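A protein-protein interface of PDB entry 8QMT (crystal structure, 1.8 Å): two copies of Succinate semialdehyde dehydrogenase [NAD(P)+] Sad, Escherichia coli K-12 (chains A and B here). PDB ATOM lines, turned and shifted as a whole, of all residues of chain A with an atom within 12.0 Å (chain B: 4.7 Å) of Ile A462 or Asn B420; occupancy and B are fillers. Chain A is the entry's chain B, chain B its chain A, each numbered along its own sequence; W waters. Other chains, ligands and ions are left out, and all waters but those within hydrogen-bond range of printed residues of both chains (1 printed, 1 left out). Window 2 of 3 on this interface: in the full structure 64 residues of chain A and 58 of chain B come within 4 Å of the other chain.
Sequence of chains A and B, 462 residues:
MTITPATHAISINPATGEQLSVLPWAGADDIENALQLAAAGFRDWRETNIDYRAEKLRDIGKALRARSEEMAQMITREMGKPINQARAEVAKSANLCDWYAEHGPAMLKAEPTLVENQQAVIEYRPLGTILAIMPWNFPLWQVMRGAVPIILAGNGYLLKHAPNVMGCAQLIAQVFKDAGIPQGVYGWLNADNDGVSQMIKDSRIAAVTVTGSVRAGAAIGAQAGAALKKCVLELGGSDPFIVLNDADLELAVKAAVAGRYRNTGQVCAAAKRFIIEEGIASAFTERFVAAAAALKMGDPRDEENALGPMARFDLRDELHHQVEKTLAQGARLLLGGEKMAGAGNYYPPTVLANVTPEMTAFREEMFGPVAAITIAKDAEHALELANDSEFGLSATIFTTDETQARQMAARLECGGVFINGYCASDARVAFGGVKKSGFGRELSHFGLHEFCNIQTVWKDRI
The backbone carbonyl oxygen (O) of Ile B397 lies within hydrogen-bond range of the backbone NH (N) of Asn B420 (2.8 Å). The backbone carbonyl oxygen (O) of Gln A119 sits at hydrogen-bond distance from the backbone NH (N) of Lys A459 (2.8 Å). NE1 of Trp A458 is in hydrogen-bond range of OE1 of Gln A119. The backbone NH (N) of Ile B397 is in hydrogen-bond range of the backbone carbonyl oxygen (O) of Phe B418 (2.9 Å). The side-chain amide nitrogen (ND2) of Asn B420 lies within hydrogen-bond range of the backbone carbonyl oxygen (O) of Thr B399. The side-chain amide nitrogen (NE2) of Gln A119 lies within hydrogen-bond range of the backbone carbonyl oxygen (O) of Asp A460, 2.9 Å away.
O of Trp A458 touches CA of Phe B418, at 3.3 Å. Lys A459 touches Ile B419 (CA to O, 3.5 Å). Asn B420 touches Asp A460 (O to CA, 3.5 Å). Arg A461 touches Phe B418 (CD to CE2, 3.8 Å). O of Arg A461 touches CA of Gly B421 (3.3 Å). CG2 of Ile A462 touches O of Asn B420, 3.6 Å away. Ile A462 touches Gly B421.
N of Asp A460 sits at hydrogen-bond distance from O of Ile B419, at 2.8 Å. The backbone carbonyl oxygen (O) of Trp A458 is in hydrogen-bond range of the backbone NH (N) of Ile B419, 2.9 Å away. N of Tyr B422 lies within hydrogen-bond range of O of Arg A461, at 2.8 Å.
Gln A119 touches none of the printed residues of chain B. Of the printed residues of chain B, Arg A461 touches Phe B418, Gly B421 and Tyr B422. Printed residues of chain B within 4 Å of Ile A462: Asn B420 and Gly B421. Ile B397 touches none of the printed residues of chain A. No residue of chain A comes within 4 Å of Thr B399. Of the printed residues of chain A, Phe B418 touches Trp A458 and Arg A461. Asn B420 touches two residues of chain A. Of the printed residues of chain A, Tyr B422 touches Arg A461 (2.8 Å). The nearest printed residue of chain B that does not touch Ile A462 is Leu B251 (4.04 Å). The nearest printed residue of chain B that does not touch Arg A461 is Asn B420 (4.2 Å).
Water W1 bridges OD1 of Asp A460 (2.6 Å) and O of Asn B420 (2.9 Å).
No position is printed for both chains. Of the 10 pairs that touch across the chains among the printed residues, none has its exchanged pair printed and touching as well.
Of the 13 printed residues of chain A, 5 touch a printed residue of chain B. Hydrophobic or aromatic side chains of chain A that line the printed part of chain B: Trp A458 and Ile A462. Among the printed residues, 10 pairs touch across the chains. Among the printed residues, no Asp or Glu carboxylate lies within 4 Å of a Lys or Arg side-chain nitrogen of the other chain.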
ATOM      1  N   VAL A 115      12.444   3.190  23.088  1.00  0.00           N
ATOM      2  CA  VAL A 115      12.994   4.194  23.992  1.00  0.00           C
ATOM      3  C   VAL A 115      13.204   5.491  23.220  1.00  0.00           C
ATOM      4  O   VAL A 115      13.616   5.486  22.053  1.00  0.00           O
ATOM      5  CB  VAL A 115      14.302   3.705  24.640  1.00  0.00           C
ATOM      6  CG1 VAL A 115      14.931   4.806  25.517  1.00  0.00           C
ATOM      7  CG2 VAL A 115      14.047   2.458  25.473  1.00  0.00           C
ATOM      8  N   GLU A 116      12.887   6.609  23.863  1.00  0.00           N
ATOM      9  CA  GLU A 116      12.991   7.908  23.212  1.00  0.00           C
ATOM     10  C   GLU A 116      14.433   8.216  22.809  1.00  0.00           C
ATOM     11  O   GLU A 116      15.393   7.775  23.449  1.00  0.00           O
ATOM     12  CB  GLU A 116      12.461   8.996  24.142  1.00  0.00           C
ATOM     13  CG  GLU A 116      13.188   9.077  25.484  1.00  0.00           C
ATOM     14  CD  GLU A 116      12.647   8.105  26.533  1.00  0.00           C
ATOM     15  OE1 GLU A 116      11.641   7.407  26.256  1.00  0.00           O
ATOM     16  OE2 GLU A 116      13.229   8.051  27.639  1.00  0.00           O
ATOM     17  N   ASN A 117      14.573   8.968  21.712  1.00  0.00           N
ATOM     18  CA  ASN A 117      15.851   9.560  21.292  1.00  0.00           C
ATOM     19  C   ASN A 117      16.904   8.510  20.957  1.00  0.00           C
ATOM     20  O   ASN A 117      18.103   8.765  21.100  1.00  0.00           O
ATOM     21  CB  ASN A 117      16.393  10.521  22.353  1.00  0.00           C
ATOM     22  CG  ASN A 117      15.404  11.619  22.698  1.00  0.00           C
ATOM     23  OD1 ASN A 117      15.095  11.855  23.871  1.00  0.00           O
ATOM     24  ND2 ASN A 117      14.894  12.292  21.677  1.00  0.00           N
ATOM     25  N   GLN A 118      16.462   7.330  20.518  1.00  0.00           N
ATOM     26  CA  GLN A 118      17.353   6.243  20.110  1.00  0.00           C
ATOM     27  C   GLN A 118      18.423   5.978  21.168  1.00  0.00           C
ATOM     28  O   GLN A 118      19.616   5.864  20.878  1.00  0.00           O
ATOM     29  CB  GLN A 118      17.973   6.540  18.744  1.00  0.00           C
ATOM     30  CG  GLN A 118      16.980   6.420  17.594  1.00  0.00           C
ATOM     31  CD  GLN A 118      17.571   6.822  16.257  1.00  0.00           C
ATOM     32  OE1 GLN A 118      18.492   7.637  16.191  1.00  0.00           O
ATOM     33  NE2 GLN A 118      17.043   6.249  15.178  1.00  0.00           N
ATOM     34  N   GLN A 119      17.980   5.895  22.421  1.00  0.00           N
ATOM     35  CA  GLN A 119      18.901   5.653  23.524  1.00  0.00           C
ATOM     36  C   GLN A 119      19.284   4.185  23.648  1.00  0.00           C
ATOM     37  O   GLN A 119      20.372   3.877  24.150  1.00  0.00           O
ATOM     38  CB  GLN A 119      18.285   6.115  24.845  1.00  0.00           C
ATOM     39  CG  GLN A 119      18.314   7.608  25.070  1.00  0.00           C
ATOM     40  CD  GLN A 119      17.963   7.975  26.501  1.00  0.00           C
ATOM     41  OE1 GLN A 119      17.184   7.282  27.171  1.00  0.00           O
ATOM     42  NE2 GLN A 119      18.553   9.058  26.986  1.00  0.00           N
ATOM     43  N   ALA A 120      18.407   3.279  23.221  1.00  0.00           N
ATOM     44  CA  ALA A 120      18.557   1.856  23.494  1.00  0.00           C
ATOM     45  C   ALA A 120      18.392   1.044  22.217  1.00  0.00           C
ATOM     46  O   ALA A 120      17.537   1.346  21.382  1.00  0.00           O
ATOM     47  CB  ALA A 120      17.534   1.387  24.543  1.00  0.00           C
ATOM     48  N   THR A 456      20.522  -5.869  25.797  1.00  0.00           N
ATOM     49  CA  THR A 456      20.101  -4.481  25.766  1.00  0.00           C
ATOM     50  C   THR A 456      21.314  -3.577  25.991  1.00  0.00           C
ATOM     51  O   THR A 456      22.072  -3.776  26.941  1.00  0.00           O
ATOM     52  CB  THR A 456      19.055  -4.230  26.854  1.00  0.00           C
ATOM     53  OG1 THR A 456      17.859  -4.970  26.572  1.00  0.00           O
ATOM     54  CG2 THR A 456      18.739  -2.733  26.985  1.00  0.00           C
ATOM     55  N   VAL A 457      21.497  -2.584  25.127  1.00  0.00           N
ATOM     56  CA  VAL A 457      22.532  -1.572  25.312  1.00  0.00           C
ATOM     57  C   VAL A 457      21.837  -0.219  25.310  1.00  0.00           C
ATOM     58  O   VAL A 457      21.214   0.166  24.313  1.00  0.00           O
ATOM     59  CB  VAL A 457      23.622  -1.646  24.233  1.00  0.00           C
ATOM     60  CG1 VAL A 457      24.775  -0.692  24.576  1.00  0.00           C
ATOM     61  CG2 VAL A 457      24.133  -3.070  24.106  1.00  0.00           C
ATOM     62  N   TRP A 458      21.923   0.487  26.435  1.00  0.00           N
ATOM     63  CA  TRP A 458      21.116   1.670  26.694  1.00  0.00           C
ATOM     64  C   TRP A 458      22.051   2.780  27.143  1.00  0.00           C
ATOM     65  O   TRP A 458      22.724   2.647  28.170  1.00  0.00           O
ATOM     66  CB  TRP A 458      20.063   1.369  27.763  1.00  0.00           C
ATOM     67  CG  TRP A 458      18.958   2.363  27.914  1.00  0.00           C
ATOM     68  CD1 TRP A 458      18.988   3.694  27.609  1.00  0.00           C
ATOM     69  CD2 TRP A 458      17.645   2.095  28.424  1.00  0.00           C
ATOM     70  NE1 TRP A 458      17.765   4.271  27.895  1.00  0.00           N
ATOM     71  CE2 TRP A 458      16.929   3.311  28.404  1.00  0.00           C
ATOM     72  CE3 TRP A 458      17.010   0.943  28.904  1.00  0.00           C
ATOM     73  CZ2 TRP A 458      15.603   3.408  28.837  1.00  0.00           C
ATOM     74  CZ3 TRP A 458      15.684   1.041  29.335  1.00  0.00           C
ATOM     75  CH2 TRP A 458      15.002   2.269  29.303  1.00  0.00           C
ATOM     76  N   LYS A 459      22.092   3.864  26.376  1.00  0.00           N
ATOM     77  CA  LYS A 459      22.972   4.993  26.651  1.00  0.00           C
ATOM     78  C   LYS A 459      22.192   6.125  27.311  1.00  0.00           C
ATOM     79  O   LYS A 459      21.068   6.430  26.908  1.00  0.00           O
ATOM     80  CB  LYS A 459      23.618   5.478  25.349  1.00  0.00           C
ATOM     81  CG  LYS A 459      24.518   6.692  25.484  1.00  0.00           C
ATOM     82  CD  LYS A 459      25.175   7.026  24.144  1.00  0.00           C
ATOM     83  CE  LYS A 459      24.141   7.169  23.037  1.00  0.00           C
ATOM     84  NZ  LYS A 459      24.791   7.504  21.738  1.00  0.00           N
ATOM     85  N   ASP A 460      22.794   6.737  28.334  1.00  0.00           N
ATOM     86  CA  ASP A 460      22.279   7.971  28.937  1.00  0.00           C
ATOM     87  C   ASP A 460      20.887   7.799  29.542  1.00  0.00           C
ATOM     88  O   ASP A 460      20.036   8.686  29.427  1.00  0.00           O
ATOM     89  CB  ASP A 460      22.261   9.121  27.922  1.00  0.00           C
ATOM     90  CG  ASP A 460      23.629   9.428  27.366  1.00  0.00           C
ATOM     91  OD1 ASP A 460      24.609   9.360  28.132  1.00  0.00           O
ATOM     92  OD2 ASP A 460      23.719   9.704  26.150  1.00  0.00           O
ATOM     93  N   ARG A 461      20.640   6.666  30.198  1.00  0.00           N
ATOM     94  CA  ARG A 461      19.361   6.502  30.888  1.00  0.00           C
ATOM     95  C   ARG A 461      19.440   7.286  32.192  1.00  0.00           C
ATOM     96  O   ARG A 461      19.892   6.778  33.220  1.00  0.00           O
ATOM     97  CB  ARG A 461      19.033   5.033  31.132  1.00  0.00           C
ATOM     98  CG  ARG A 461      17.616   4.851  31.647  1.00  0.00           C
ATOM     99  CD  ARG A 461      17.290   3.441  32.113  1.00  0.00           C
ATOM    100  NE  ARG A 461      15.981   3.431  32.753  1.00  0.00           N
ATOM    101  CZ  ARG A 461      15.754   3.723  34.028  1.00  0.00           C
ATOM    102  NH1 ARG A 461      16.747   3.985  34.869  1.00  0.00           N
ATOM    103  NH2 ARG A 461      14.500   3.757  34.473  1.00  0.00           N
ATOM    104  N   ILE A 462      19.010   8.548  32.139  1.00  0.00           N
ATOM    105  CA  ILE A 462      19.068   9.451  33.284  1.00  0.00           C
ATOM    106  C   ILE A 462      17.777  10.251  33.388  1.00  0.00           C
ATOM    107  O   ILE A 462      16.932  10.210  32.497  1.00  0.00           O
ATOM    108  CB  ILE A 462      20.283  10.407  33.200  1.00  0.00           C
ATOM    109  CG1 ILE A 462      20.199  11.274  31.938  1.00  0.00           C
ATOM    110  CG2 ILE A 462      21.601   9.636  33.259  1.00  0.00           C
ATOM    111  CD1 ILE A 462      21.265  12.376  31.883  1.00  0.00           C
ATOM    112  OXT ILE A 462      17.543  10.960  34.370  1.00  0.00           O
ATOM    113  N   LEU B 251      27.763  12.257  38.293  1.00  0.00           N
ATOM    114  CA  LEU B 251      26.682  11.387  37.832  1.00  0.00           C
ATOM    115  C   LEU B 251      26.986   9.920  38.112  1.00  0.00           C
ATOM    116  O   LEU B 251      26.082   9.142  38.446  1.00  0.00           O
ATOM    117  CB  LEU B 251      26.445  11.602  36.338  1.00  0.00           C
ATOM    118  CG  LEU B 251      25.263  10.884  35.684  1.00  0.00           C
ATOM    119  CD1 LEU B 251      23.962  11.225  36.392  1.00  0.00           C
ATOM    120  CD2 LEU B 251      25.177  11.257  34.220  1.00  0.00           C
ATOM    121  N   ILE B 397      28.731   1.114  32.502  1.00  0.00           N
ATOM    122  CA  ILE B 397      30.011   1.719  32.145  1.00  0.00           C
ATOM    123  C   ILE B 397      29.856   3.224  32.197  1.00  0.00           C
ATOM    124  O   ILE B 397      29.012   3.784  31.490  1.00  0.00           O
ATOM    125  CB  ILE B 397      30.486   1.311  30.743  1.00  0.00           C
ATOM    126  CG1 ILE B 397      30.458  -0.203  30.570  1.00  0.00           C
ATOM    127  CG2 ILE B 397      31.892   1.847  30.511  1.00  0.00           C
ATOM    128  CD1 ILE B 397      30.710  -0.648  29.128  1.00  0.00           C
ATOM    129  N   PHE B 398      30.693   3.885  33.004  1.00  0.00           N
ATOM    130  CA  PHE B 398      30.774   5.342  33.027  1.00  0.00           C
ATOM    131  C   PHE B 398      32.099   5.764  32.396  1.00  0.00           C
ATOM    132  O   PHE B 398      33.174   5.454  32.922  1.00  0.00           O
ATOM    133  CB  PHE B 398      30.616   5.888  34.447  1.00  0.00           C
ATOM    134  CG  PHE B 398      29.220   6.308  34.753  1.00  0.00           C
ATOM    135  CD1 PHE B 398      28.284   5.381  35.194  1.00  0.00           C
ATOM    136  CD2 PHE B 398      28.818   7.616  34.542  1.00  0.00           C
ATOM    137  CE1 PHE B 398      26.983   5.757  35.443  1.00  0.00           C
ATOM    138  CE2 PHE B 398      27.521   7.999  34.790  1.00  0.00           C
ATOM    139  CZ  PHE B 398      26.598   7.072  35.242  1.00  0.00           C
ATOM    140  N   THR B 399      32.007   6.436  31.250  1.00  0.00           N
ATOM    141  CA  THR B 399      33.145   7.008  30.543  1.00  0.00           C
ATOM    142  C   THR B 399      32.610   7.983  29.506  1.00  0.00           C
ATOM    143  O   THR B 399      31.555   7.741  28.910  1.00  0.00           O
ATOM    144  CB  THR B 399      34.008   5.932  29.865  1.00  0.00           C
ATOM    145  OG1 THR B 399      35.012   6.562  29.062  1.00  0.00           O
ATOM    146  CG2 THR B 399      33.159   5.031  28.970  1.00  0.00           C
ATOM    147  N   PHE B 418      24.395  -0.571  30.493  1.00  0.00           N
ATOM    148  CA  PHE B 418      23.958   0.813  30.599  1.00  0.00           C
ATOM    149  C   PHE B 418      25.192   1.692  30.556  1.00  0.00           C
ATOM    150  O   PHE B 418      26.123   1.497  31.339  1.00  0.00           O
ATOM    151  CB  PHE B 418      23.134   1.037  31.870  1.00  0.00           C
ATOM    152  CG  PHE B 418      21.809   0.362  31.804  1.00  0.00           C
ATOM    153  CD1 PHE B 418      21.711  -1.004  32.023  1.00  0.00           C
ATOM    154  CD2 PHE B 418      20.680   1.063  31.415  1.00  0.00           C
ATOM    155  CE1 PHE B 418      20.493  -1.648  31.910  1.00  0.00           C
ATOM    156  CE2 PHE B 418      19.458   0.423  31.293  1.00  0.00           C
ATOM    157  CZ  PHE B 418      19.364  -0.930  31.545  1.00  0.00           C
ATOM    158  N   ILE B 419      25.216   2.611  29.601  1.00  0.00           N
ATOM    159  CA  ILE B 419      26.344   3.507  29.399  1.00  0.00           C
ATOM    160  C   ILE B 419      25.943   4.863  29.964  1.00  0.00           C
ATOM    161  O   ILE B 419      24.970   5.469  29.503  1.00  0.00           O
ATOM    162  CB  ILE B 419      26.729   3.594  27.912  1.00  0.00           C
ATOM    163  CG1 ILE B 419      27.121   2.201  27.395  1.00  0.00           C
ATOM    164  CG2 ILE B 419      27.868   4.587  27.714  1.00  0.00           C
ATOM    165  CD1 ILE B 419      27.334   2.106  25.877  1.00  0.00           C
ATOM    166  N   ASN B 420      26.662   5.304  30.993  1.00  0.00           N
ATOM    167  CA  ASN B 420      26.458   6.617  31.617  1.00  0.00           C
ATOM    168  C   ASN B 420      25.004   6.820  32.039  1.00  0.00           C
ATOM    169  O   ASN B 420      24.389   7.846  31.746  1.00  0.00           O
ATOM    170  CB  ASN B 420      26.909   7.742  30.681  1.00  0.00           C
ATOM    171  CG  ASN B 420      28.380   7.656  30.331  1.00  0.00           C
ATOM    172  OD1 ASN B 420      29.213   7.357  31.182  1.00  0.00           O
ATOM    173  ND2 ASN B 420      28.706   7.913  29.068  1.00  0.00           N
ATOM    174  N   GLY B 421      24.448   5.829  32.727  1.00  0.00           N
ATOM    175  CA  GLY B 421      23.070   5.921  33.156  1.00  0.00           C
ATOM    176  C   GLY B 421      22.727   4.916  34.237  1.00  0.00           C
ATOM    177  O   GLY B 421      23.592   4.187  34.733  1.00  0.00           O
ATOM    178  N   TYR B 422      21.433   4.879  34.574  1.00  0.00           N
ATOM    179  CA  TYR B 422      20.897   4.077  35.671  1.00  0.00           C
ATOM    180  C   TYR B 422      20.321   2.777  35.124  1.00  0.00           C
ATOM    181  O   TYR B 422      19.339   2.800  34.374  1.00  0.00           O
ATOM    182  CB  TYR B 422      19.799   4.833  36.419  1.00  0.00           C
ATOM    183  CG  TYR B 422      20.241   6.072  37.172  1.00  0.00           C
ATOM    184  CD1 TYR B 422      20.493   7.260  36.504  1.00  0.00           C
ATOM    185  CD2 TYR B 422      20.352   6.063  38.554  1.00  0.00           C
ATOM    186  CE1 TYR B 422      20.874   8.403  37.191  1.00  0.00           C
ATOM    187  CE2 TYR B 422      20.727   7.214  39.257  1.00  0.00           C
ATOM    188  CZ  TYR B 422      20.991   8.376  38.566  1.00  0.00           C
ATOM    189  OH  TYR B 422      21.365   9.522  39.244  1.00  0.00           O
HETATM  190  O   HOH W   1      24.397  10.432  30.491  1.00  0.00           O
